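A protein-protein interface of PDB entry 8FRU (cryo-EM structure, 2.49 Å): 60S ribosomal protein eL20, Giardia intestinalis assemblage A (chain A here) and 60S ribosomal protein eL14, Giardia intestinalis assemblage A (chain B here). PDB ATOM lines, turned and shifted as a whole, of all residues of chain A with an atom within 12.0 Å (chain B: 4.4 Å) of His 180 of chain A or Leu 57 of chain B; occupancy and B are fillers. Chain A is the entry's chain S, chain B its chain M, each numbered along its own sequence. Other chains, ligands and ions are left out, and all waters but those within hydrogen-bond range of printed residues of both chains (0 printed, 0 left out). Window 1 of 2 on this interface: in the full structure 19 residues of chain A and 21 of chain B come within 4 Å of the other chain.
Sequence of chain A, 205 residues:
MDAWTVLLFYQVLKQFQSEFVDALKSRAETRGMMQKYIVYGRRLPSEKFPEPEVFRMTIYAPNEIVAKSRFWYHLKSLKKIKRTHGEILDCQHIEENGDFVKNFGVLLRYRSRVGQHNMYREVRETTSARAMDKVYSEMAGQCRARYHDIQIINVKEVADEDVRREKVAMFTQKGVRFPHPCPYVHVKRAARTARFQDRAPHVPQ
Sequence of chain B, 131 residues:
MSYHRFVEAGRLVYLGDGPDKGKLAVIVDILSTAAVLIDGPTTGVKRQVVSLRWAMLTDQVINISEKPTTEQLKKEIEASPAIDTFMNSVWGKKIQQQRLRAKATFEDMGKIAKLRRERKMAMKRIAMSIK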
ATOM      1  N   PHE A 171     -32.901 -28.076   5.499  1.00  0.00           N
ATOM      2  CA  PHE A 171     -31.865 -27.632   4.575  1.00  0.00           C
ATOM      3  C   PHE A 171     -32.409 -26.985   3.309  1.00  0.00           C
ATOM      4  O   PHE A 171     -31.616 -26.477   2.510  1.00  0.00           O
ATOM      5  CB  PHE A 171     -30.949 -28.798   4.213  1.00  0.00           C
ATOM      6  CG  PHE A 171     -29.915 -29.069   5.250  1.00  0.00           C
ATOM      7  CD1 PHE A 171     -28.935 -28.140   5.517  1.00  0.00           C
ATOM      8  CD2 PHE A 171     -29.950 -30.229   5.994  1.00  0.00           C
ATOM      9  CE1 PHE A 171     -27.995 -28.375   6.484  1.00  0.00           C
ATOM     10  CE2 PHE A 171     -29.010 -30.465   6.960  1.00  0.00           C
ATOM     11  CZ  PHE A 171     -28.032 -29.537   7.206  1.00  0.00           C
ATOM     12  N   VAL A 176     -29.495 -20.274   5.327  1.00  0.00           N
ATOM     13  CA  VAL A 176     -29.181 -21.234   6.378  1.00  0.00           C
ATOM     14  C   VAL A 176     -27.688 -21.193   6.672  1.00  0.00           C
ATOM     15  O   VAL A 176     -26.859 -21.153   5.755  1.00  0.00           O
ATOM     16  CB  VAL A 176     -29.645 -22.643   5.967  1.00  0.00           C
ATOM     17  CG1 VAL A 176     -29.401 -22.870   4.491  1.00  0.00           C
ATOM     18  CG2 VAL A 176     -28.947 -23.701   6.796  1.00  0.00           C
ATOM     19  N   ARG A 177     -27.340 -21.183   7.958  1.00  0.00           N
ATOM     20  CA  ARG A 177     -25.961 -21.057   8.404  1.00  0.00           C
ATOM     21  C   ARG A 177     -25.699 -22.025   9.543  1.00  0.00           C
ATOM     22  O   ARG A 177     -26.607 -22.373  10.299  1.00  0.00           O
ATOM     23  CB  ARG A 177     -25.646 -19.639   8.894  1.00  0.00           C
ATOM     24  CG  ARG A 177     -25.658 -18.581   7.830  1.00  0.00           C
ATOM     25  CD  ARG A 177     -25.950 -17.214   8.431  1.00  0.00           C
ATOM     26  NE  ARG A 177     -24.752 -16.589   8.978  1.00  0.00           N
ATOM     27  CZ  ARG A 177     -24.498 -16.458  10.272  1.00  0.00           C
ATOM     28  NH1 ARG A 177     -25.351 -16.879  11.189  1.00  0.00           N
ATOM     29  NH2 ARG A 177     -23.358 -15.890  10.654  1.00  0.00           N
ATOM     30  N   PHE A 178     -24.450 -22.452   9.666  1.00  0.00           N
ATOM     31  CA  PHE A 178     -24.004 -23.200  10.833  1.00  0.00           C
ATOM     32  C   PHE A 178     -22.483 -23.263  10.809  1.00  0.00           C
ATOM     33  O   PHE A 178     -21.874 -23.094   9.756  1.00  0.00           O
ATOM     34  CB  PHE A 178     -24.611 -24.612  10.878  1.00  0.00           C
ATOM     35  CG  PHE A 178     -24.496 -25.382   9.594  1.00  0.00           C
ATOM     36  CD1 PHE A 178     -23.392 -26.172   9.344  1.00  0.00           C
ATOM     37  CD2 PHE A 178     -25.508 -25.345   8.657  1.00  0.00           C
ATOM     38  CE1 PHE A 178     -23.291 -26.890   8.181  1.00  0.00           C
ATOM     39  CE2 PHE A 178     -25.408 -26.060   7.488  1.00  0.00           C
ATOM     40  CZ  PHE A 178     -24.301 -26.834   7.251  1.00  0.00           C
ATOM     41  N   PRO A 179     -21.862 -23.473  11.961  1.00  0.00           N
ATOM     42  CA  PRO A 179     -20.404 -23.600  12.016  1.00  0.00           C
ATOM     43  C   PRO A 179     -19.937 -24.955  11.499  1.00  0.00           C
ATOM     44  O   PRO A 179     -20.710 -25.896  11.340  1.00  0.00           O
ATOM     45  CB  PRO A 179     -20.096 -23.435  13.508  1.00  0.00           C
ATOM     46  CG  PRO A 179     -21.350 -23.778  14.202  1.00  0.00           C
ATOM     47  CD  PRO A 179     -22.469 -23.414  13.299  1.00  0.00           C
ATOM     48  N   HIS A 180     -18.636 -25.038  11.245  1.00  0.00           N
ATOM     49  CA  HIS A 180     -18.057 -26.255  10.693  1.00  0.00           C
ATOM     50  C   HIS A 180     -18.316 -27.431  11.630  1.00  0.00           C
ATOM     51  O   HIS A 180     -18.004 -27.349  12.822  1.00  0.00           O
ATOM     52  CB  HIS A 180     -16.558 -26.078  10.469  1.00  0.00           C
ATOM     53  CG  HIS A 180     -15.967 -27.071   9.518  1.00  0.00           C
ATOM     54  ND1 HIS A 180     -16.088 -28.431   9.693  1.00  0.00           N
ATOM     55  CD2 HIS A 180     -15.256 -26.902   8.380  1.00  0.00           C
ATOM     56  CE1 HIS A 180     -15.475 -29.056   8.707  1.00  0.00           C
ATOM     57  NE2 HIS A 180     -14.962 -28.151   7.897  1.00  0.00           N
ATOM     58  N   PRO A 181     -18.880 -28.535  11.135  1.00  0.00           N
ATOM     59  CA  PRO A 181     -19.295 -29.618  12.040  1.00  0.00           C
ATOM     60  C   PRO A 181     -18.150 -30.440  12.612  1.00  0.00           C
ATOM     61  O   PRO A 181     -18.360 -31.127  13.616  1.00  0.00           O
ATOM     62  CB  PRO A 181     -20.206 -30.488  11.163  1.00  0.00           C
ATOM     63  CG  PRO A 181     -20.444 -29.723   9.921  1.00  0.00           C
ATOM     64  CD  PRO A 181     -19.345 -28.744   9.757  1.00  0.00           C
ATOM     65  N   CYS A 182     -16.956 -30.408  12.022  1.00  0.00           N
ATOM     66  CA  CYS A 182     -15.848 -31.254  12.467  1.00  0.00           C
ATOM     67  C   CYS A 182     -14.526 -30.621  12.061  1.00  0.00           C
ATOM     68  O   CYS A 182     -13.791 -31.153  11.224  1.00  0.00           O
ATOM     69  CB  CYS A 182     -15.978 -32.661  11.888  1.00  0.00           C
ATOM     70  SG  CYS A 182     -16.313 -32.714  10.117  1.00  0.00           S
ATOM     71  N   PRO A 183     -14.173 -29.483  12.662  1.00  0.00           N
ATOM     72  CA  PRO A 183     -12.896 -28.845  12.317  1.00  0.00           C
ATOM     73  C   PRO A 183     -11.682 -29.559  12.892  1.00  0.00           C
ATOM     74  O   PRO A 183     -10.561 -29.286  12.447  1.00  0.00           O
ATOM     75  CB  PRO A 183     -13.041 -27.428  12.889  1.00  0.00           C
ATOM     76  CG  PRO A 183     -14.302 -27.420  13.686  1.00  0.00           C
ATOM     77  CD  PRO A 183     -14.852 -28.797  13.767  1.00  0.00           C
ATOM     78  N   TYR A 184     -11.865 -30.465  13.853  1.00  0.00           N
ATOM     79  CA  TYR A 184     -10.740 -31.230  14.372  1.00  0.00           C
ATOM     80  C   TYR A 184     -10.129 -32.140  13.314  1.00  0.00           C
ATOM     81  O   TYR A 184      -8.959 -32.517  13.436  1.00  0.00           O
ATOM     82  CB  TYR A 184     -11.186 -32.050  15.584  1.00  0.00           C
ATOM     83  CG  TYR A 184     -12.169 -33.140  15.243  1.00  0.00           C
ATOM     84  CD1 TYR A 184     -13.531 -32.897  15.229  1.00  0.00           C
ATOM     85  CD2 TYR A 184     -11.731 -34.410  14.922  1.00  0.00           C
ATOM     86  CE1 TYR A 184     -14.423 -33.889  14.909  1.00  0.00           C
ATOM     87  CE2 TYR A 184     -12.612 -35.403  14.602  1.00  0.00           C
ATOM     88  CZ  TYR A 184     -13.955 -35.142  14.592  1.00  0.00           C
ATOM     89  OH  TYR A 184     -14.827 -36.152  14.269  1.00  0.00           O
ATOM     90  N   VAL A 185     -10.892 -32.491  12.276  1.00  0.00           N
ATOM     91  CA  VAL A 185     -10.411 -33.417  11.257  1.00  0.00           C
ATOM     92  C   VAL A 185      -9.240 -32.822  10.486  1.00  0.00           C
ATOM     93  O   VAL A 185      -8.306 -33.536  10.112  1.00  0.00           O
ATOM     94  CB  VAL A 185     -11.559 -33.815  10.316  1.00  0.00           C
ATOM     95  CG1 VAL A 185     -11.066 -34.766   9.256  1.00  0.00           C
ATOM     96  CG2 VAL A 185     -12.694 -34.445  11.096  1.00  0.00           C
ATOM     97  N   HIS A 186      -9.277 -31.518  10.213  1.00  0.00           N
ATOM     98  CA  HIS A 186      -8.173 -30.890   9.496  1.00  0.00           C
ATOM     99  C   HIS A 186      -6.882 -30.966  10.294  1.00  0.00           C
ATOM    100  O   HIS A 186      -5.821 -31.280   9.746  1.00  0.00           O
ATOM    101  CB  HIS A 186      -8.512 -29.437   9.172  1.00  0.00           C
ATOM    102  CG  HIS A 186      -9.843 -29.259   8.519  1.00  0.00           C
ATOM    103  ND1 HIS A 186     -10.138 -29.777   7.279  1.00  0.00           N
ATOM    104  CD2 HIS A 186     -10.965 -28.633   8.941  1.00  0.00           C
ATOM    105  CE1 HIS A 186     -11.383 -29.477   6.963  1.00  0.00           C
ATOM    106  NE2 HIS A 186     -11.907 -28.783   7.955  1.00  0.00           N
ATOM    107  N   VAL A 187      -6.952 -30.672  11.593  1.00  0.00           N
ATOM    108  CA  VAL A 187      -5.763 -30.716  12.435  1.00  0.00           C
ATOM    109  C   VAL A 187      -5.261 -32.143  12.577  1.00  0.00           C
ATOM    110  O   VAL A 187      -4.054 -32.397  12.540  1.00  0.00           O
ATOM    111  CB  VAL A 187      -6.059 -30.082  13.804  1.00  0.00           C
ATOM    112  CG1 VAL A 187      -4.830 -30.109  14.676  1.00  0.00           C
ATOM    113  CG2 VAL A 187      -6.549 -28.667  13.627  1.00  0.00           C
ATOM    114  N   LYS A 188      -6.178 -33.094  12.747  1.00  0.00           N
ATOM    115  CA  LYS A 188      -5.781 -34.491  12.867  1.00  0.00           C
ATOM    116  C   LYS A 188      -5.102 -34.981  11.597  1.00  0.00           C
ATOM    117  O   LYS A 188      -4.099 -35.697  11.655  1.00  0.00           O
ATOM    118  CB  LYS A 188      -7.006 -35.341  13.192  1.00  0.00           C
ATOM    119  CG  LYS A 188      -6.746 -36.500  14.116  1.00  0.00           C
ATOM    120  CD  LYS A 188      -7.926 -37.450  14.129  1.00  0.00           C
ATOM    121  CE  LYS A 188      -8.000 -38.225  15.430  1.00  0.00           C
ATOM    122  NZ  LYS A 188      -9.400 -38.567  15.792  1.00  0.00           N
ATOM    123  N   ARG A 189      -5.626 -34.588  10.438  1.00  0.00           N
ATOM    124  CA  ARG A 189      -5.088 -35.063   9.168  1.00  0.00           C
ATOM    125  C   ARG A 189      -3.641 -34.622   8.971  1.00  0.00           C
ATOM    126  O   ARG A 189      -2.828 -35.373   8.424  1.00  0.00           O
ATOM    127  CB  ARG A 189      -5.973 -34.563   8.024  1.00  0.00           C
ATOM    128  CG  ARG A 189      -5.584 -35.056   6.645  1.00  0.00           C
ATOM    129  CD  ARG A 189      -6.056 -34.097   5.559  1.00  0.00           C
ATOM    130  NE  ARG A 189      -7.492 -33.857   5.617  1.00  0.00           N
ATOM    131  CZ  ARG A 189      -8.048 -32.656   5.687  1.00  0.00           C
ATOM    132  NH1 ARG A 189      -7.318 -31.558   5.734  1.00  0.00           N
ATOM    133  NH2 ARG A 189      -9.373 -32.557   5.717  1.00  0.00           N
ATOM    134  N   HIS A 202      -3.940 -25.290  17.640  1.00  0.00           N
ATOM    135  CA  HIS A 202      -5.307 -24.910  17.953  1.00  0.00           C
ATOM    136  C   HIS A 202      -6.239 -25.272  16.802  1.00  0.00           C
ATOM    137  O   HIS A 202      -5.815 -25.476  15.664  1.00  0.00           O
ATOM    138  CB  HIS A 202      -5.403 -23.416  18.242  1.00  0.00           C
ATOM    139  CG  HIS A 202      -4.860 -23.023  19.577  1.00  0.00           C
ATOM    140  ND1 HIS A 202      -4.220 -21.825  19.793  1.00  0.00           N
ATOM    141  CD2 HIS A 202      -4.868 -23.665  20.767  1.00  0.00           C
ATOM    142  CE1 HIS A 202      -3.854 -21.747  21.058  1.00  0.00           C
ATOM    143  NE2 HIS A 202      -4.234 -22.853  21.671  1.00  0.00           N
ATOM    144  N   VAL A 203      -7.527 -25.333  17.115  1.00  0.00           N
ATOM    145  CA  VAL A 203      -8.557 -25.645  16.130  1.00  0.00           C
ATOM    146  C   VAL A 203      -9.293 -24.358  15.780  1.00  0.00           C
ATOM    147  O   VAL A 203     -10.121 -23.889  16.573  1.00  0.00           O
ATOM    148  CB  VAL A 203      -9.527 -26.707  16.667  1.00  0.00           C
ATOM    149  CG1 VAL A 203     -10.337 -27.309  15.544  1.00  0.00           C
ATOM    150  CG2 VAL A 203      -8.771 -27.777  17.418  1.00  0.00           C
ATOM    151  N   PRO A 204      -9.037 -23.757  14.620  1.00  0.00           N
ATOM    152  CA  PRO A 204      -9.699 -22.491  14.291  1.00  0.00           C
ATOM    153  C   PRO A 204     -11.168 -22.707  13.975  1.00  0.00           C
ATOM    154  O   PRO A 204     -11.553 -23.716  13.382  1.00  0.00           O
ATOM    155  CB  PRO A 204      -8.927 -21.991  13.063  1.00  0.00           C
ATOM    156  CG  PRO A 204      -7.750 -22.901  12.922  1.00  0.00           C
ATOM    157  CD  PRO A 204      -8.145 -24.193  13.541  1.00  0.00           C
ATOM    158  N   GLN A 205     -11.989 -21.741  14.372  1.00  0.00           N
ATOM    159  CA  GLN A 205     -13.432 -21.851  14.200  1.00  0.00           C
ATOM    160  C   GLN A 205     -14.053 -20.502  13.858  1.00  0.00           C
ATOM    161  O   GLN A 205     -13.619 -19.465  14.354  1.00  0.00           O
ATOM    162  CB  GLN A 205     -14.080 -22.418  15.464  1.00  0.00           C
ATOM    163  CG  GLN A 205     -13.384 -23.630  16.025  1.00  0.00           C
ATOM    164  CD  GLN A 205     -14.352 -24.668  16.542  1.00  0.00           C
ATOM    165  OE1 GLN A 205     -15.374 -24.945  15.921  1.00  0.00           O
ATOM    166  NE2 GLN A 205     -14.034 -25.247  17.690  1.00  0.00           N
ATOM    167  N   ARG B   5     -16.592 -17.946  11.773  1.00  0.00           N
ATOM    168  CA  ARG B   5     -16.707 -18.385  10.389  1.00  0.00           C
ATOM    169  C   ARG B   5     -17.756 -19.482  10.291  1.00  0.00           C
ATOM    170  O   ARG B   5     -17.755 -20.420  11.093  1.00  0.00           O
ATOM    171  CB  ARG B   5     -15.360 -18.864   9.846  1.00  0.00           C
ATOM    172  CG  ARG B   5     -14.437 -19.453  10.876  1.00  0.00           C
ATOM    173  CD  ARG B   5     -13.077 -19.758  10.283  1.00  0.00           C
ATOM    174  NE  ARG B   5     -12.179 -18.610  10.295  1.00  0.00           N
ATOM    175  CZ  ARG B   5     -10.863 -18.694  10.146  1.00  0.00           C
ATOM    176  NH1 ARG B   5     -10.261 -19.857   9.968  1.00  0.00           N
ATOM    177  NH2 ARG B   5     -10.134 -17.585  10.180  1.00  0.00           N
ATOM    178  N   PHE B   6     -18.648 -19.358   9.311  1.00  0.00           N
ATOM    179  CA  PHE B   6     -19.801 -20.232   9.176  1.00  0.00           C
ATOM    180  C   PHE B   6     -19.863 -20.830   7.780  1.00  0.00           C
ATOM    181  O   PHE B   6     -19.456 -20.206   6.801  1.00  0.00           O
ATOM    182  CB  PHE B   6     -21.100 -19.480   9.439  1.00  0.00           C
ATOM    183  CG  PHE B   6     -21.318 -19.129  10.876  1.00  0.00           C
ATOM    184  CD1 PHE B   6     -20.612 -18.099  11.465  1.00  0.00           C
ATOM    185  CD2 PHE B   6     -22.242 -19.821  11.632  1.00  0.00           C
ATOM    186  CE1 PHE B   6     -20.816 -17.774  12.777  1.00  0.00           C
ATOM    187  CE2 PHE B   6     -22.448 -19.500  12.944  1.00  0.00           C
ATOM    188  CZ  PHE B   6     -21.736 -18.475  13.518  1.00  0.00           C
ATOM    189  N   VAL B   7     -20.396 -22.047   7.698  1.00  0.00           N
ATOM    190  CA  VAL B   7     -20.712 -22.656   6.410  1.00  0.00           C
ATOM    191  C   VAL B   7     -21.939 -21.940   5.854  1.00  0.00           C
ATOM    192  O   VAL B   7     -23.033 -22.049   6.410  1.00  0.00           O
ATOM    193  CB  VAL B   7     -20.965 -24.161   6.545  1.00  0.00           C
ATOM    194  CG1 VAL B   7     -21.373 -24.744   5.213  1.00  0.00           C
ATOM    195  CG2 VAL B   7     -19.744 -24.866   7.081  1.00  0.00           C
ATOM    196  N   ARG B  11     -19.222 -18.247   1.066  1.00  0.00           N
ATOM    197  CA  ARG B  11     -18.029 -18.360   1.891  1.00  0.00           C
ATOM    198  C   ARG B  11     -16.871 -18.926   1.081  1.00  0.00           C
ATOM    199  O   ARG B  11     -17.035 -19.877   0.313  1.00  0.00           O
ATOM    200  CB  ARG B  11     -18.316 -19.247   3.098  1.00  0.00           C
ATOM    201  CG  ARG B  11     -17.123 -20.008   3.614  1.00  0.00           C
ATOM    202  CD  ARG B  11     -16.435 -19.242   4.719  1.00  0.00           C
ATOM    203  NE  ARG B  11     -17.394 -18.700   5.671  1.00  0.00           N
ATOM    204  CZ  ARG B  11     -17.146 -17.687   6.486  1.00  0.00           C
ATOM    205  NH1 ARG B  11     -15.978 -17.072   6.485  1.00  0.00           N
ATOM    206  NH2 ARG B  11     -18.095 -17.280   7.320  1.00  0.00           N
ATOM    207  N   LEU B  12     -15.697 -18.326   1.243  1.00  0.00           N
ATOM    208  CA  LEU B  12     -14.499 -18.809   0.573  1.00  0.00           C
ATOM    209  C   LEU B  12     -13.906 -19.979   1.344  1.00  0.00           C
ATOM    210  O   LEU B  12     -13.895 -19.987   2.576  1.00  0.00           O
ATOM    211  CB  LEU B  12     -13.475 -17.687   0.439  1.00  0.00           C
ATOM    212  CG  LEU B  12     -12.281 -17.945  -0.473  1.00  0.00           C
ATOM    213  CD1 LEU B  12     -12.739 -18.102  -1.906  1.00  0.00           C
ATOM    214  CD2 LEU B  12     -11.284 -16.814  -0.356  1.00  0.00           C
ATOM    215  N   VAL B  13     -13.407 -20.970   0.612  1.00  0.00           N
ATOM    216  CA  VAL B  13     -13.026 -22.248   1.194  1.00  0.00           C
ATOM    217  C   VAL B  13     -11.700 -22.700   0.602  1.00  0.00           C
ATOM    218  O   VAL B  13     -11.435 -22.502  -0.586  1.00  0.00           O
ATOM    219  CB  VAL B  13     -14.128 -23.305   0.968  1.00  0.00           C
ATOM    220  CG1 VAL B  13     -13.727 -24.283  -0.112  1.00  0.00           C
ATOM    221  CG2 VAL B  13     -14.449 -24.017   2.258  1.00  0.00           C
ATOM    222  N   LEU B  52     -17.561 -31.896   3.676  1.00  0.00           N
ATOM    223  CA  LEU B  52     -17.018 -30.812   4.481  1.00  0.00           C
ATOM    224  C   LEU B  52     -15.747 -31.204   5.214  1.00  0.00           C
ATOM    225  O   LEU B  52     -15.053 -30.323   5.727  1.00  0.00           O
ATOM    226  CB  LEU B  52     -18.067 -30.333   5.478  1.00  0.00           C
ATOM    227  CG  LEU B  52     -18.977 -29.232   4.940  1.00  0.00           C
ATOM    228  CD1 LEU B  52     -20.326 -29.261   5.633  1.00  0.00           C
ATOM    229  CD2 LEU B  52     -18.312 -27.889   5.109  1.00  0.00           C
ATOM    230  N   ALA B  55     -12.908 -29.315   3.277  1.00  0.00           N
ATOM    231  CA  ALA B  55     -12.898 -27.872   3.089  1.00  0.00           C
ATOM    232  C   ALA B  55     -12.607 -27.156   4.401  1.00  0.00           C
ATOM    233  O   ALA B  55     -13.309 -27.357   5.393  1.00  0.00           O
ATOM    234  CB  ALA B  55     -14.240 -27.402   2.527  1.00  0.00           C
ATOM    235  N   MET B  56     -11.584 -26.308   4.392  1.00  0.00           N
ATOM    236  CA  MET B  56     -11.244 -25.459   5.526  1.00  0.00           C
ATOM    237  C   MET B  56     -11.814 -24.064   5.299  1.00  0.00           C
ATOM    238  O   MET B  56     -11.540 -23.436   4.274  1.00  0.00           O
ATOM    239  CB  MET B  56      -9.730 -25.388   5.722  1.00  0.00           C
ATOM    240  CG  MET B  56      -9.049 -26.735   5.864  1.00  0.00           C
ATOM    241  SD  MET B  56      -7.248 -26.646   5.754  1.00  0.00           S
ATOM    242  CE  MET B  56      -6.821 -26.032   7.377  1.00  0.00           C
ATOM    243  N   LEU B  57     -12.604 -23.587   6.255  1.00  0.00           N
ATOM    244  CA  LEU B  57     -13.280 -22.308   6.094  1.00  0.00           C
ATOM    245  C   LEU B  57     -12.303 -21.149   6.227  1.00  0.00           C
ATOM    246  O   LEU B  57     -11.407 -21.159   7.071  1.00  0.00           O
ATOM    247  CB  LEU B  57     -14.396 -22.162   7.125  1.00  0.00           C
ATOM    248  CG  LEU B  57     -15.382 -23.320   7.257  1.00  0.00           C
ATOM    249  CD1 LEU B  57     -16.521 -22.926   8.168  1.00  0.00           C
ATOM    250  CD2 LEU B  57     -15.898 -23.752   5.900  1.00  0.00           C
ATOM    251  N   THR B  58     -12.493 -20.142   5.389  1.00  0.00           N
ATOM    252  CA  THR B  58     -11.698 -18.926   5.380  1.00  0.00           C
ATOM    253  C   THR B  58     -12.493 -17.796   6.027  1.00  0.00           C
ATOM    254  O   THR B  58     -13.683 -17.928   6.316  1.00  0.00           O
ATOM    255  CB  THR B  58     -11.302 -18.582   3.938  1.00  0.00           C
ATOM    256  OG1 THR B  58     -10.394 -19.572   3.446  1.00  0.00           O
ATOM    257  CG2 THR B  58     -10.634 -17.238   3.849  1.00  0.00           C
ATOM    258  N   TRP B  91      -1.892 -16.301   5.971  1.00  0.00           N
ATOM    259  CA  TRP B  91      -2.216 -17.597   5.391  1.00  0.00           C
ATOM    260  C   TRP B  91      -1.932 -17.620   3.894  1.00  0.00           C
ATOM    261  O   TRP B  91      -1.408 -18.610   3.373  1.00  0.00           O
ATOM    262  CB  TRP B  91      -3.675 -17.937   5.677  1.00  0.00           C
ATOM    263  CG  TRP B  91      -3.970 -19.389   5.613  1.00  0.00           C
ATOM    264  CD1 TRP B  91      -3.083 -20.390   5.383  1.00  0.00           C
ATOM    265  CD2 TRP B  91      -5.243 -20.011   5.778  1.00  0.00           C
ATOM    266  NE1 TRP B  91      -3.720 -21.598   5.395  1.00  0.00           N
ATOM    267  CE2 TRP B  91      -5.052 -21.393   5.635  1.00  0.00           C
ATOM    268  CE3 TRP B  91      -6.529 -19.533   6.038  1.00  0.00           C
ATOM    269  CZ2 TRP B  91      -6.094 -22.301   5.740  1.00  0.00           C
ATOM    270  CZ3 TRP B  91      -7.558 -20.434   6.138  1.00  0.00           C
ATOM    271  CH2 TRP B  91      -7.339 -21.802   5.990  1.00  0.00           C
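A ring nitrogen (NE2) of His 186 of chain A lies within hydrogen-bond range of a ring nitrogen (NE2) of His 180 of chain A (3.1 Å).
The backbone carbonyl oxygen (O) of Phe 6 of chain B sits at hydrogen-bond distance from the guanidinium group (NE) of Arg 11 of chain B, at 2.8 Å.
The backbone carbonyl oxygen (O) of Leu 57 of chain B lies within hydrogen-bond range of the guanidinium group (NH1) of Arg 5 of chain B (3.4 Å).
ND1 of His 186 of chain A sits at hydrogen-bond distance from NH2 of Arg 189 of chain A (3.3 Å).
N of Cys 182 of chain A sits at hydrogen-bond distance from ND1 of His 180 of chain A (3.2 Å).
Val 7 of chain B touches Val 176 of chain A (O to O, 3.98 Å).
Phe 6 of chain B touches Arg 177 of chain A.
Val 7 of chain B touches Arg 177 of chain A.
Phe 6 of chain B touches Phe 178 of chain A (CD2 to C, 3.5 Å).
Phe 6 of chain B touches Pro 179 of chain A (CD2 to N, 3.7 Å).
His 180 of chain A touches Leu 57 of chain B.
His 186 of chain A touches Leu 52 of chain B.
His 186 of chain A touches Met 56 of chain B (ND1 to CG, 3.5 Å).
Arg 5 of chain B touches Pro 204 of chain A (NH1 to CB, 3.99 Å).
Arg 5 of chain B touches Gln 205 of chain A.
Of the 12 printed residues of chain B, 7 touch a printed residue of chain A.
Printed residues of chain B that touch a printed residue of chain A: Arg 5, Phe 6, Val 7, Leu 52, Ala 55, Met 56 and Leu 57.
Hydrophobic or aromatic side chains of chain B that line the printed part of chain A: Phe 6, Val 7, Met 56 and Leu 57.
Along chain B the printed residues that touch a printed residue of chain A span positions 5 to 57.
Of the 19 printed residues of chain A, 8 touch a printed residue of chain B.
Printed residues of chain A that touch a printed residue of chain B: Val 176, Arg 177, Phe 178, Pro 179, His 180, His 186, Pro 204 and Gln 205.
Hydrophobic or aromatic side chains of chain A that line the printed part of chain B: Phe 178, Pro 179, His 180, His 186 and Pro 204.
Among the printed residues, 14 pairs touch across the chains.
Among the printed residues, no Asp or Glu carboxylate lies within 4 Å of a Lys or Arg side-chain nitrogen of the other chain.
The backbone carbonyl oxygen (O) of Leu 52 of chain B sits at hydrogen-bond distance from a ring nitrogen (NE2) of His 180 of chain A (3.1 Å).
The backbone carbonyl oxygen (O) of Ala 55 of chain B sits at hydrogen-bond distance from a ring nitrogen (NE2) of His 186 of chain A, 3.3 Å away.
NE2 of His 180 of chain A lies within hydrogen-bond range of O of Ala 55 of chain B, at 3.1 Å.
The backbone NH (N) of Val 7 of chain B sits at hydrogen-bond distance from the backbone carbonyl oxygen (O) of Phe 178 of chain A (2.7 Å).
Of chain A, only His 180 comes within 4 Å of Leu 57 of chain B.
Of chain A, only Arg 177, Phe 178 and Pro 179 come within 4 Å of Phe 6 of chain B.
No residue of chain A comes within 4 Å of Val 13 of chain B.
Of chain A, only His 180 (3.1 Å) and His 186 (3.3 Å) come within 4 Å of Ala 55 of chain B.
Met 56 of chain B touches just one residue of chain A: His 186 (3.5 Å).
No residue of chain A comes within 4 Å of Thr 58 of chain B.
Of the printed residues of chain A, Arg 5 of chain B touches Pro 204 and Gln 205.
Printed residues of chain B within 4 Å of Pro 179 of chain A: Phe 6.
Printed residues of chain B within 4 Å of Val 176 of chain A: Val 7 (3.98 Å).
Of the printed residues of chain B, His 186 of chain A touches Leu 52 (3.96 Å), Ala 55 (3.3 Å) and Met 56 (3.5 Å).
Printed residues of chain A within 4 Å of Val 7 of chain B: Val 176, Arg 177 and Phe 178.
Tyr 184 of chain A touches none of the printed residues of chain B.
The nearest residue of chain B that does not touch His 180 of chain A is Val 7 of chain B (4.2 Å).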
